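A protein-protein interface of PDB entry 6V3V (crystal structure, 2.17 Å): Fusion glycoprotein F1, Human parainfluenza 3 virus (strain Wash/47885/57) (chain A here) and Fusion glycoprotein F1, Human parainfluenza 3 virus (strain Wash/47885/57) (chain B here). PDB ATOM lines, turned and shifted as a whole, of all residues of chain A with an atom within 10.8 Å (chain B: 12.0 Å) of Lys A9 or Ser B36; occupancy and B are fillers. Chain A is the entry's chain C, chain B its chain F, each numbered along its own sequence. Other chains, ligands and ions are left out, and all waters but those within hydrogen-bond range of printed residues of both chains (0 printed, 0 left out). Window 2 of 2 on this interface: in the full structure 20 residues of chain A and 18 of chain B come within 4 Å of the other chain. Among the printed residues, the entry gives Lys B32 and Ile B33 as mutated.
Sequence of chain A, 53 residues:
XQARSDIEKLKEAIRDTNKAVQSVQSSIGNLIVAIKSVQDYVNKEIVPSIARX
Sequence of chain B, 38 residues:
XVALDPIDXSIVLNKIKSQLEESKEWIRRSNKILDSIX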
ATOM      1  N   ARG A   4      31.292  15.724  -1.593  1.00  0.00           N
ATOM      2  CA  ARG A   4      32.405  15.184  -2.365  1.00  0.00           C
ATOM      3  C   ARG A   4      32.718  13.753  -1.940  1.00  0.00           C
ATOM      4  O   ARG A   4      33.427  13.027  -2.637  1.00  0.00           O
ATOM      5  CB  ARG A   4      33.648  16.065  -2.206  1.00  0.00           C
ATOM      6  N   SER A   5      32.180  13.356  -0.791  1.00  0.00           N
ATOM      7  CA  SER A   5      32.396  12.011  -0.281  1.00  0.00           C
ATOM      8  C   SER A   5      31.649  10.985  -1.132  1.00  0.00           C
ATOM      9  O   SER A   5      30.665  11.294  -1.809  1.00  0.00           O
ATOM     10  CB  SER A   5      31.924  11.920   1.171  1.00  0.00           C
ATOM     11  OG  SER A   5      32.082  10.608   1.681  1.00  0.00           O
ATOM     12  N   ASP A   6      32.136   9.742  -1.090  1.00  0.00           N
ATOM     13  CA  ASP A   6      31.500   8.672  -1.854  1.00  0.00           C
ATOM     14  C   ASP A   6      30.100   8.372  -1.336  1.00  0.00           C
ATOM     15  O   ASP A   6      29.172   8.161  -2.127  1.00  0.00           O
ATOM     16  CB  ASP A   6      32.365   7.411  -1.831  1.00  0.00           C
ATOM     17  CG  ASP A   6      33.391   7.387  -2.947  1.00  0.00           C
ATOM     18  OD1 ASP A   6      33.381   8.312  -3.787  1.00  0.00           O
ATOM     19  OD2 ASP A   6      34.206   6.441  -2.984  1.00  0.00           O
ATOM     20  N   ILE A   7      29.929   8.338  -0.012  1.00  0.00           N
ATOM     21  CA  ILE A   7      28.600   8.138   0.561  1.00  0.00           C
ATOM     22  C   ILE A   7      27.672   9.274   0.155  1.00  0.00           C
ATOM     23  O   ILE A   7      26.492   9.057  -0.147  1.00  0.00           O
ATOM     24  CB  ILE A   7      28.691   7.974   2.090  1.00  0.00           C
ATOM     25  CG1 ILE A   7      29.439   6.685   2.439  1.00  0.00           C
ATOM     26  CG2 ILE A   7      27.303   7.980   2.718  1.00  0.00           C
ATOM     27  CD1 ILE A   7      29.594   6.452   3.927  1.00  0.00           C
ATOM     28  N   GLU A   8      28.196  10.504   0.126  1.00  0.00           N
ATOM     29  CA  GLU A   8      27.404  11.633  -0.346  1.00  0.00           C
ATOM     30  C   GLU A   8      27.030  11.465  -1.814  1.00  0.00           C
ATOM     31  O   GLU A   8      25.879  11.701  -2.197  1.00  0.00           O
ATOM     32  CB  GLU A   8      28.168  12.940  -0.130  1.00  0.00           C
ATOM     33  N   LYS A   9      27.987  11.049  -2.649  1.00  0.00           N
ATOM     34  CA  LYS A   9      27.691  10.824  -4.061  1.00  0.00           C
ATOM     35  C   LYS A   9      26.657   9.717  -4.241  1.00  0.00           C
ATOM     36  O   LYS A   9      25.740   9.842  -5.062  1.00  0.00           O
ATOM     37  CB  LYS A   9      28.976  10.499  -4.822  1.00  0.00           C
ATOM     38  CG  LYS A   9      29.929  11.675  -4.964  1.00  0.00           C
ATOM     39  CD  LYS A   9      31.242  11.246  -5.597  1.00  0.00           C
ATOM     40  CE  LYS A   9      32.209  12.416  -5.704  1.00  0.00           C
ATOM     41  NZ  LYS A   9      33.597  11.970  -6.018  1.00  0.00           N
ATOM     42  N   LEU A  10      26.788   8.625  -3.481  1.00  0.00           N
ATOM     43  CA  LEU A  10      25.783   7.566  -3.534  1.00  0.00           C
ATOM     44  C   LEU A  10      24.415   8.081  -3.106  1.00  0.00           C
ATOM     45  O   LEU A  10      23.401   7.769  -3.739  1.00  0.00           O
ATOM     46  CB  LEU A  10      26.211   6.391  -2.653  1.00  0.00           C
ATOM     47  CG  LEU A  10      27.323   5.483  -3.180  1.00  0.00           C
ATOM     48  CD1 LEU A  10      27.819   4.557  -2.080  1.00  0.00           C
ATOM     49  CD2 LEU A  10      26.831   4.680  -4.374  1.00  0.00           C
ATOM     50  N   LYS A  11      24.369   8.876  -2.034  1.00  0.00           N
ATOM     51  CA  LYS A  11      23.096   9.404  -1.551  1.00  0.00           C
ATOM     52  C   LYS A  11      22.429  10.295  -2.591  1.00  0.00           C
ATOM     53  O   LYS A  11      21.214  10.207  -2.807  1.00  0.00           O
ATOM     54  CB  LYS A  11      23.316  10.166  -0.244  1.00  0.00           C
ATOM     55  CG  LYS A  11      22.136  11.018   0.198  1.00  0.00           C
ATOM     56  CD  LYS A  11      22.493  11.854   1.421  1.00  0.00           C
ATOM     57  CE  LYS A  11      21.383  12.835   1.765  1.00  0.00           C
ATOM     58  NZ  LYS A  11      21.747  13.712   2.908  1.00  0.00           N
ATOM     59  N   GLU A  12      23.205  11.159  -3.251  1.00  0.00           N
ATOM     60  CA  GLU A  12      22.616  12.072  -4.227  1.00  0.00           C
ATOM     61  C   GLU A  12      22.180  11.346  -5.494  1.00  0.00           C
ATOM     62  O   GLU A  12      21.204  11.757  -6.133  1.00  0.00           O
ATOM     63  CB  GLU A  12      23.580  13.213  -4.556  1.00  0.00           C
ATOM     64  CG  GLU A  12      24.097  13.969  -3.339  1.00  0.00           C
ATOM     65  CD  GLU A  12      22.996  14.383  -2.378  1.00  0.00           C
ATOM     66  OE1 GLU A  12      21.918  14.816  -2.843  1.00  0.00           O
ATOM     67  OE2 GLU A  12      23.213  14.277  -1.152  1.00  0.00           O
ATOM     68  N   ALA A  13      22.880  10.274  -5.873  1.00  0.00           N
ATOM     69  CA  ALA A  13      22.466   9.502  -7.040  1.00  0.00           C
ATOM     70  C   ALA A  13      21.099   8.866  -6.820  1.00  0.00           C
ATOM     71  O   ALA A  13      20.251   8.874  -7.721  1.00  0.00           O
ATOM     72  CB  ALA A  13      23.512   8.439  -7.373  1.00  0.00           C
ATOM     73  N   ILE A  14      20.865   8.313  -5.627  1.00  0.00           N
ATOM     74  CA  ILE A  14      19.560   7.730  -5.330  1.00  0.00           C
ATOM     75  C   ILE A  14      18.481   8.803  -5.316  1.00  0.00           C
ATOM     76  O   ILE A  14      17.329   8.539  -5.687  1.00  0.00           O
ATOM     77  CB  ILE A  14      19.604   6.930  -4.017  1.00  0.00           C
ATOM     78  CG1 ILE A  14      20.782   5.957  -4.022  1.00  0.00           C
ATOM     79  CG2 ILE A  14      18.298   6.177  -3.802  1.00  0.00           C
ATOM     80  CD1 ILE A  14      21.097   5.389  -2.663  1.00  0.00           C
ATOM     81  N   ARG A  15      18.825  10.025  -4.895  1.00  0.00           N
ATOM     82  CA  ARG A  15      17.861  11.119  -4.948  1.00  0.00           C
ATOM     83  C   ARG A  15      17.411  11.376  -6.380  1.00  0.00           C
ATOM     84  O   ARG A  15      16.212  11.496  -6.652  1.00  0.00           O
ATOM     85  CB  ARG A  15      18.455  12.384  -4.328  1.00  0.00           C
ATOM     86  CG  ARG A  15      18.636  12.296  -2.828  1.00  0.00           C
ATOM     87  CD  ARG A  15      17.329  11.915  -2.153  1.00  0.00           C
ATOM     88  NE  ARG A  15      16.481  13.067  -1.871  1.00  0.00           N
ATOM     89  CZ  ARG A  15      16.460  13.701  -0.705  1.00  0.00           C
ATOM     90  NH1 ARG A  15      15.655  14.739  -0.527  1.00  0.00           N
ATOM     91  NH2 ARG A  15      17.246  13.297   0.285  1.00  0.00           N
ATOM     92  N   ASP A  16      18.365  11.460  -7.310  1.00  0.00           N
ATOM     93  CA  ASP A  16      18.022  11.631  -8.718  1.00  0.00           C
ATOM     94  C   ASP A  16      17.194  10.459  -9.224  1.00  0.00           C
ATOM     95  O   ASP A  16      16.189  10.647  -9.921  1.00  0.00           O
ATOM     96  CB  ASP A  16      19.297  11.779  -9.548  1.00  0.00           C
ATOM     97  CG  ASP A  16      20.101  13.002  -9.166  1.00  0.00           C
ATOM     98  OD1 ASP A  16      19.568  13.857  -8.429  1.00  0.00           O
ATOM     99  OD2 ASP A  16      21.267  13.110  -9.603  1.00  0.00           O
ATOM    100  N   THR A  17      17.604   9.235  -8.881  1.00  0.00           N
ATOM    101  CA  THR A  17      16.848   8.056  -9.290  1.00  0.00           C
ATOM    102  C   THR A  17      15.425   8.096  -8.746  1.00  0.00           C
ATOM    103  O   THR A  17      14.471   7.778  -9.464  1.00  0.00           O
ATOM    104  CB  THR A  17      17.568   6.792  -8.825  1.00  0.00           C
ATOM    105  OG1 THR A  17      18.907   6.789  -9.341  1.00  0.00           O
ATOM    106  CG2 THR A  17      16.832   5.544  -9.309  1.00  0.00           C
ATOM    107  N   TRP B  26      16.428  12.985 -15.239  1.00  0.00           N
ATOM    108  CA  TRP B  26      16.768  12.659 -13.857  1.00  0.00           C
ATOM    109  C   TRP B  26      17.659  11.426 -13.776  1.00  0.00           C
ATOM    110  O   TRP B  26      18.568  11.365 -12.940  1.00  0.00           O
ATOM    111  CB  TRP B  26      15.501  12.475 -13.020  1.00  0.00           C
ATOM    112  CG  TRP B  26      14.885  13.761 -12.552  1.00  0.00           C
ATOM    113  CD1 TRP B  26      13.705  14.304 -12.966  1.00  0.00           C
ATOM    114  CD2 TRP B  26      15.422  14.665 -11.577  1.00  0.00           C
ATOM    115  NE1 TRP B  26      13.472  15.490 -12.311  1.00  0.00           N
ATOM    116  CE2 TRP B  26      14.512  15.734 -11.452  1.00  0.00           C
ATOM    117  CE3 TRP B  26      16.581  14.673 -10.797  1.00  0.00           C
ATOM    118  CZ2 TRP B  26      14.727  16.800 -10.582  1.00  0.00           C
ATOM    119  CZ3 TRP B  26      16.791  15.732  -9.932  1.00  0.00           C
ATOM    120  CH2 TRP B  26      15.870  16.780  -9.831  1.00  0.00           C
ATOM    121  N   ILE B  27      17.411  10.430 -14.629  1.00  0.00           N
ATOM    122  CA  ILE B  27      18.299   9.271 -14.683  1.00  0.00           C
ATOM    123  C   ILE B  27      19.679   9.677 -15.186  1.00  0.00           C
ATOM    124  O   ILE B  27      20.703   9.175 -14.704  1.00  0.00           O
ATOM    125  CB  ILE B  27      17.673   8.140 -15.522  1.00  0.00           C
ATOM    126  CG1 ILE B  27      16.539   7.475 -14.746  1.00  0.00           C
ATOM    127  CG2 ILE B  27      18.717   7.102 -15.902  1.00  0.00           C
ATOM    128  CD1 ILE B  27      16.984   6.869 -13.433  1.00  0.00           C
ATOM    129  N   ARG B  28      19.730  10.602 -16.150  1.00  0.00           N
ATOM    130  CA  ARG B  28      21.013  11.076 -16.661  1.00  0.00           C
ATOM    131  C   ARG B  28      21.853  11.706 -15.556  1.00  0.00           C
ATOM    132  O   ARG B  28      23.063  11.464 -15.475  1.00  0.00           O
ATOM    133  CB  ARG B  28      20.789  12.067 -17.804  1.00  0.00           C
ATOM    134  CG  ARG B  28      20.178  11.441 -19.047  1.00  0.00           C
ATOM    135  CD  ARG B  28      19.834  12.484 -20.100  1.00  0.00           C
ATOM    136  NE  ARG B  28      19.145  11.890 -21.244  1.00  0.00           N
ATOM    137  CZ  ARG B  28      18.631  12.587 -22.252  1.00  0.00           C
ATOM    138  NH1 ARG B  28      18.722  13.910 -22.261  1.00  0.00           N
ATOM    139  NH2 ARG B  28      18.020  11.961 -23.250  1.00  0.00           N
ATOM    140  N   ARG B  29      21.230  12.512 -14.693  1.00  0.00           N
ATOM    141  CA  ARG B  29      21.970  13.120 -13.591  1.00  0.00           C
ATOM    142  C   ARG B  29      22.427  12.074 -12.580  1.00  0.00           C
ATOM    143  O   ARG B  29      23.525  12.183 -12.023  1.00  0.00           O
ATOM    144  CB  ARG B  29      21.124  14.199 -12.915  1.00  0.00           C
ATOM    145  CG  ARG B  29      20.779  15.367 -13.818  1.00  0.00           C
ATOM    146  CD  ARG B  29      20.067  16.477 -13.057  1.00  0.00           C
ATOM    147  NE  ARG B  29      20.900  17.048 -12.000  1.00  0.00           N
ATOM    148  CZ  ARG B  29      20.802  16.727 -10.713  1.00  0.00           C
ATOM    149  NH1 ARG B  29      19.903  15.839 -10.321  1.00  0.00           N
ATOM    150  NH2 ARG B  29      21.601  17.293  -9.820  1.00  0.00           N
ATOM    151  N   SER B  30      21.598  11.058 -12.325  1.00  0.00           N
ATOM    152  CA  SER B  30      21.996   9.985 -11.420  1.00  0.00           C
ATOM    153  C   SER B  30      23.226   9.254 -11.944  1.00  0.00           C
ATOM    154  O   SER B  30      24.196   9.037 -11.209  1.00  0.00           O
ATOM    155  CB  SER B  30      20.834   9.010 -11.226  1.00  0.00           C
ATOM    156  OG  SER B  30      21.244   7.885 -10.470  1.00  0.00           O
ATOM    157  N   ASN B  31      23.203   8.869 -13.223  1.00  0.00           N
ATOM    158  CA  ASN B  31      24.359   8.208 -13.818  1.00  0.00           C
ATOM    159  C   ASN B  31      25.576   9.123 -13.849  1.00  0.00           C
ATOM    160  O   ASN B  31      26.713   8.641 -13.831  1.00  0.00           O
ATOM    161  CB  ASN B  31      24.019   7.723 -15.230  1.00  0.00           C
ATOM    162  CG  ASN B  31      23.074   6.538 -15.225  1.00  0.00           C
ATOM    163  OD1 ASN B  31      23.296   5.557 -14.515  1.00  0.00           O
ATOM    164  ND2 ASN B  31      22.008   6.625 -16.013  1.00  0.00           N
ATOM    165  N   LYS B  32      25.359  10.440 -13.887  1.00  0.00           N
ATOM    166  CA  LYS B  32      26.482  11.371 -13.942  1.00  0.00           C
ATOM    167  C   LYS B  32      27.211  11.442 -12.604  1.00  0.00           C
ATOM    168  O   LYS B  32      28.443  11.555 -12.570  1.00  0.00           O
ATOM    169  CB  LYS B  32      26.001  12.753 -14.390  1.00  0.00           C
ATOM    170  CG  LYS B  32      27.115  13.682 -14.853  1.00  0.00           C
ATOM    171  CD  LYS B  32      26.556  14.917 -15.546  1.00  0.00           C
ATOM    172  CE  LYS B  32      25.689  15.739 -14.608  1.00  0.00           C
ATOM    173  NZ  LYS B  32      25.178  16.975 -15.265  1.00  0.00           N
ATOM    174  N   ILE B  33      26.473  11.378 -11.494  1.00  0.00           N
ATOM    175  CA  ILE B  33      27.116  11.340 -10.183  1.00  0.00           C
ATOM    176  C   ILE B  33      27.904  10.048 -10.013  1.00  0.00           C
ATOM    177  O   ILE B  33      29.000  10.042  -9.440  1.00  0.00           O
ATOM    178  CB  ILE B  33      26.077  11.532  -9.062  1.00  0.00           C
ATOM    179  CG1 ILE B  33      25.322  12.848  -9.244  1.00  0.00           C
ATOM    180  CG2 ILE B  33      26.751  11.496  -7.699  1.00  0.00           C
ATOM    181  CD1 ILE B  33      24.236  13.066  -8.208  1.00  0.00           C
ATOM    182  N   LEU B  34      27.366   8.936 -10.518  1.00  0.00           N
ATOM    183  CA  LEU B  34      28.035   7.645 -10.403  1.00  0.00           C
ATOM    184  C   LEU B  34      29.355   7.590 -11.162  1.00  0.00           C
ATOM    185  O   LEU B  34      30.137   6.661 -10.938  1.00  0.00           O
ATOM    186  CB  LEU B  34      27.101   6.524 -10.869  1.00  0.00           C
ATOM    187  CG  LEU B  34      25.802   6.356 -10.076  1.00  0.00           C
ATOM    188  CD1 LEU B  34      24.867   5.364 -10.762  1.00  0.00           C
ATOM    189  CD2 LEU B  34      26.092   5.926  -8.643  1.00  0.00           C
ATOM    190  N   ASP B  35      29.623   8.552 -12.049  1.00  0.00           N
ATOM    191  CA  ASP B  35      30.920   8.596 -12.715  1.00  0.00           C
ATOM    192  C   ASP B  35      32.020   9.016 -11.749  1.00  0.00           C
ATOM    193  O   ASP B  35      33.119   8.448 -11.765  1.00  0.00           O
ATOM    194  CB  ASP B  35      30.867   9.550 -13.909  1.00  0.00           C
ATOM    195  CG  ASP B  35      29.898   9.093 -14.981  1.00  0.00           C
ATOM    196  OD1 ASP B  35      29.650   7.872 -15.081  1.00  0.00           O
ATOM    197  OD2 ASP B  35      29.386   9.954 -15.727  1.00  0.00           O
ATOM    198  N   SER B  36      31.742  10.005 -10.897  1.00  0.00           N
ATOM    199  CA  SER B  36      32.738  10.514  -9.962  1.00  0.00           C
ATOM    200  C   SER B  36      33.011   9.565  -8.803  1.00  0.00           C
ATOM    201  O   SER B  36      33.951   9.808  -8.039  1.00  0.00           O
ATOM    202  CB  SER B  36      32.303  11.879  -9.424  1.00  0.00           C
ATOM    203  N   ILE B  37      32.223   8.506  -8.650  1.00  0.00           N
ATOM    204  CA  ILE B  37      32.417   7.563  -7.554  1.00  0.00           C
ATOM    205  C   ILE B  37      33.403   6.463  -7.944  1.00  0.00           C
ATOM    206  O   ILE B  37      34.607   6.701  -8.046  1.00  0.00           O
ATOM    207  CB  ILE B  37      31.076   6.979  -7.064  1.00  0.00           C
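The backbone carbonyl oxygen (O) of Ala A13 sits at hydrogen-bond distance from the side-chain hydroxyl (OG1) of Thr A17, 3.0 Å away.
Asp A6 touches Ile B37.
Lys A9 touches Ile B33 (O to CG2, 3.3 Å).
CD1 of Ile B33 touches CB of Glu A12 (3.7 Å).
N of Ala A13 touches CD1 of Ile B33, at 3.9 Å.
CD2 of Leu B34 touches CB of Ala A13, at 3.8 Å.
Trp B26 touches Asp A16 (O to CB, 3.5 Å).
OD2 of Asp A16 touches CD1 of Ile B33 (3.3 Å).
The side-chain amino group (NZ) of Lys A9 sits at hydrogen-bond distance from the backbone carbonyl oxygen (O) of Ser B36.
O of Ala A13 sits at hydrogen-bond distance from OG of Ser B30, at 3.1 Å.
The side-chain carboxylate (OD1) of Asp A16 lies within salt-bridge range of the guanidinium group (NH1) of Arg B29.
The side-chain carboxylate (OD2) of Asp A16 sits at hydrogen-bond distance from the backbone NH (N) of Ser B30.
The side-chain hydroxyl of Ser B30 lies within hydrogen-bond range of the side-chain hydroxyl of Thr A17, at 2.8 Å.
Of the 12 printed residues of chain B, 7 touch a printed residue of chain A.
Of the 14 printed residues of chain A, 6 touch a printed residue of chain B.
Printed residues of chain A that touch a printed residue of chain B: Asp A6, Lys A9, Glu A12, Ala A13, Asp A16 and Thr A17.
Among the printed residues, Asp or Glu carboxylates within 4 Å of a Lys or Arg side-chain nitrogen of the other chain: Asp A16 with Arg B29.
Arg A4 touches none of the printed residues of chain B.
Of chain B, only Ile B37 comes within 4 Å of Asp A6.
No residue of chain B comes within 4 Å of Glu A8.
Of the printed residues of chain B, Lys A9 touches Ile B33 and Ser B36.
No residue of chain B comes within 4 Å of Leu A10.
Of chain B, only Ile B33 comes within 4 Å of Glu A12.
Ala A13 touches just these residues of chain B: Ser B30 (3.1 Å), Ile B33 (3.9 Å) and Leu B34 (3.8 Å).
Arg A15 touches none of the printed residues of chain B.
Of the printed residues of chain B, Asp A16 touches Trp B26 (3.5 Å), Arg B29 (2.8 Å), Ser B30 (3.4 Å) and Ile B33 (3.3 Å).
Printed residues of chain B within 4 Å of Thr A17: Ser B30.
Of the printed residues of chain A, Trp B26 touches Asp A16.
Ile B33 touches just these residues of chain A: Lys A9 (3.3 Å), Glu A12 (3.7 Å), Ala A13 (3.9 Å) and Asp A16 (3.3 Å).
No residue of chain A comes within 4 Å of Asp B35.
Ser B36 touches one residue of chain A.
Of chain A, only Asp A6 comes within 4 Å of Ile B37.
The nearest residue of chain B that does not touch Lys A9 is Ile B37 (4.2 Å).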
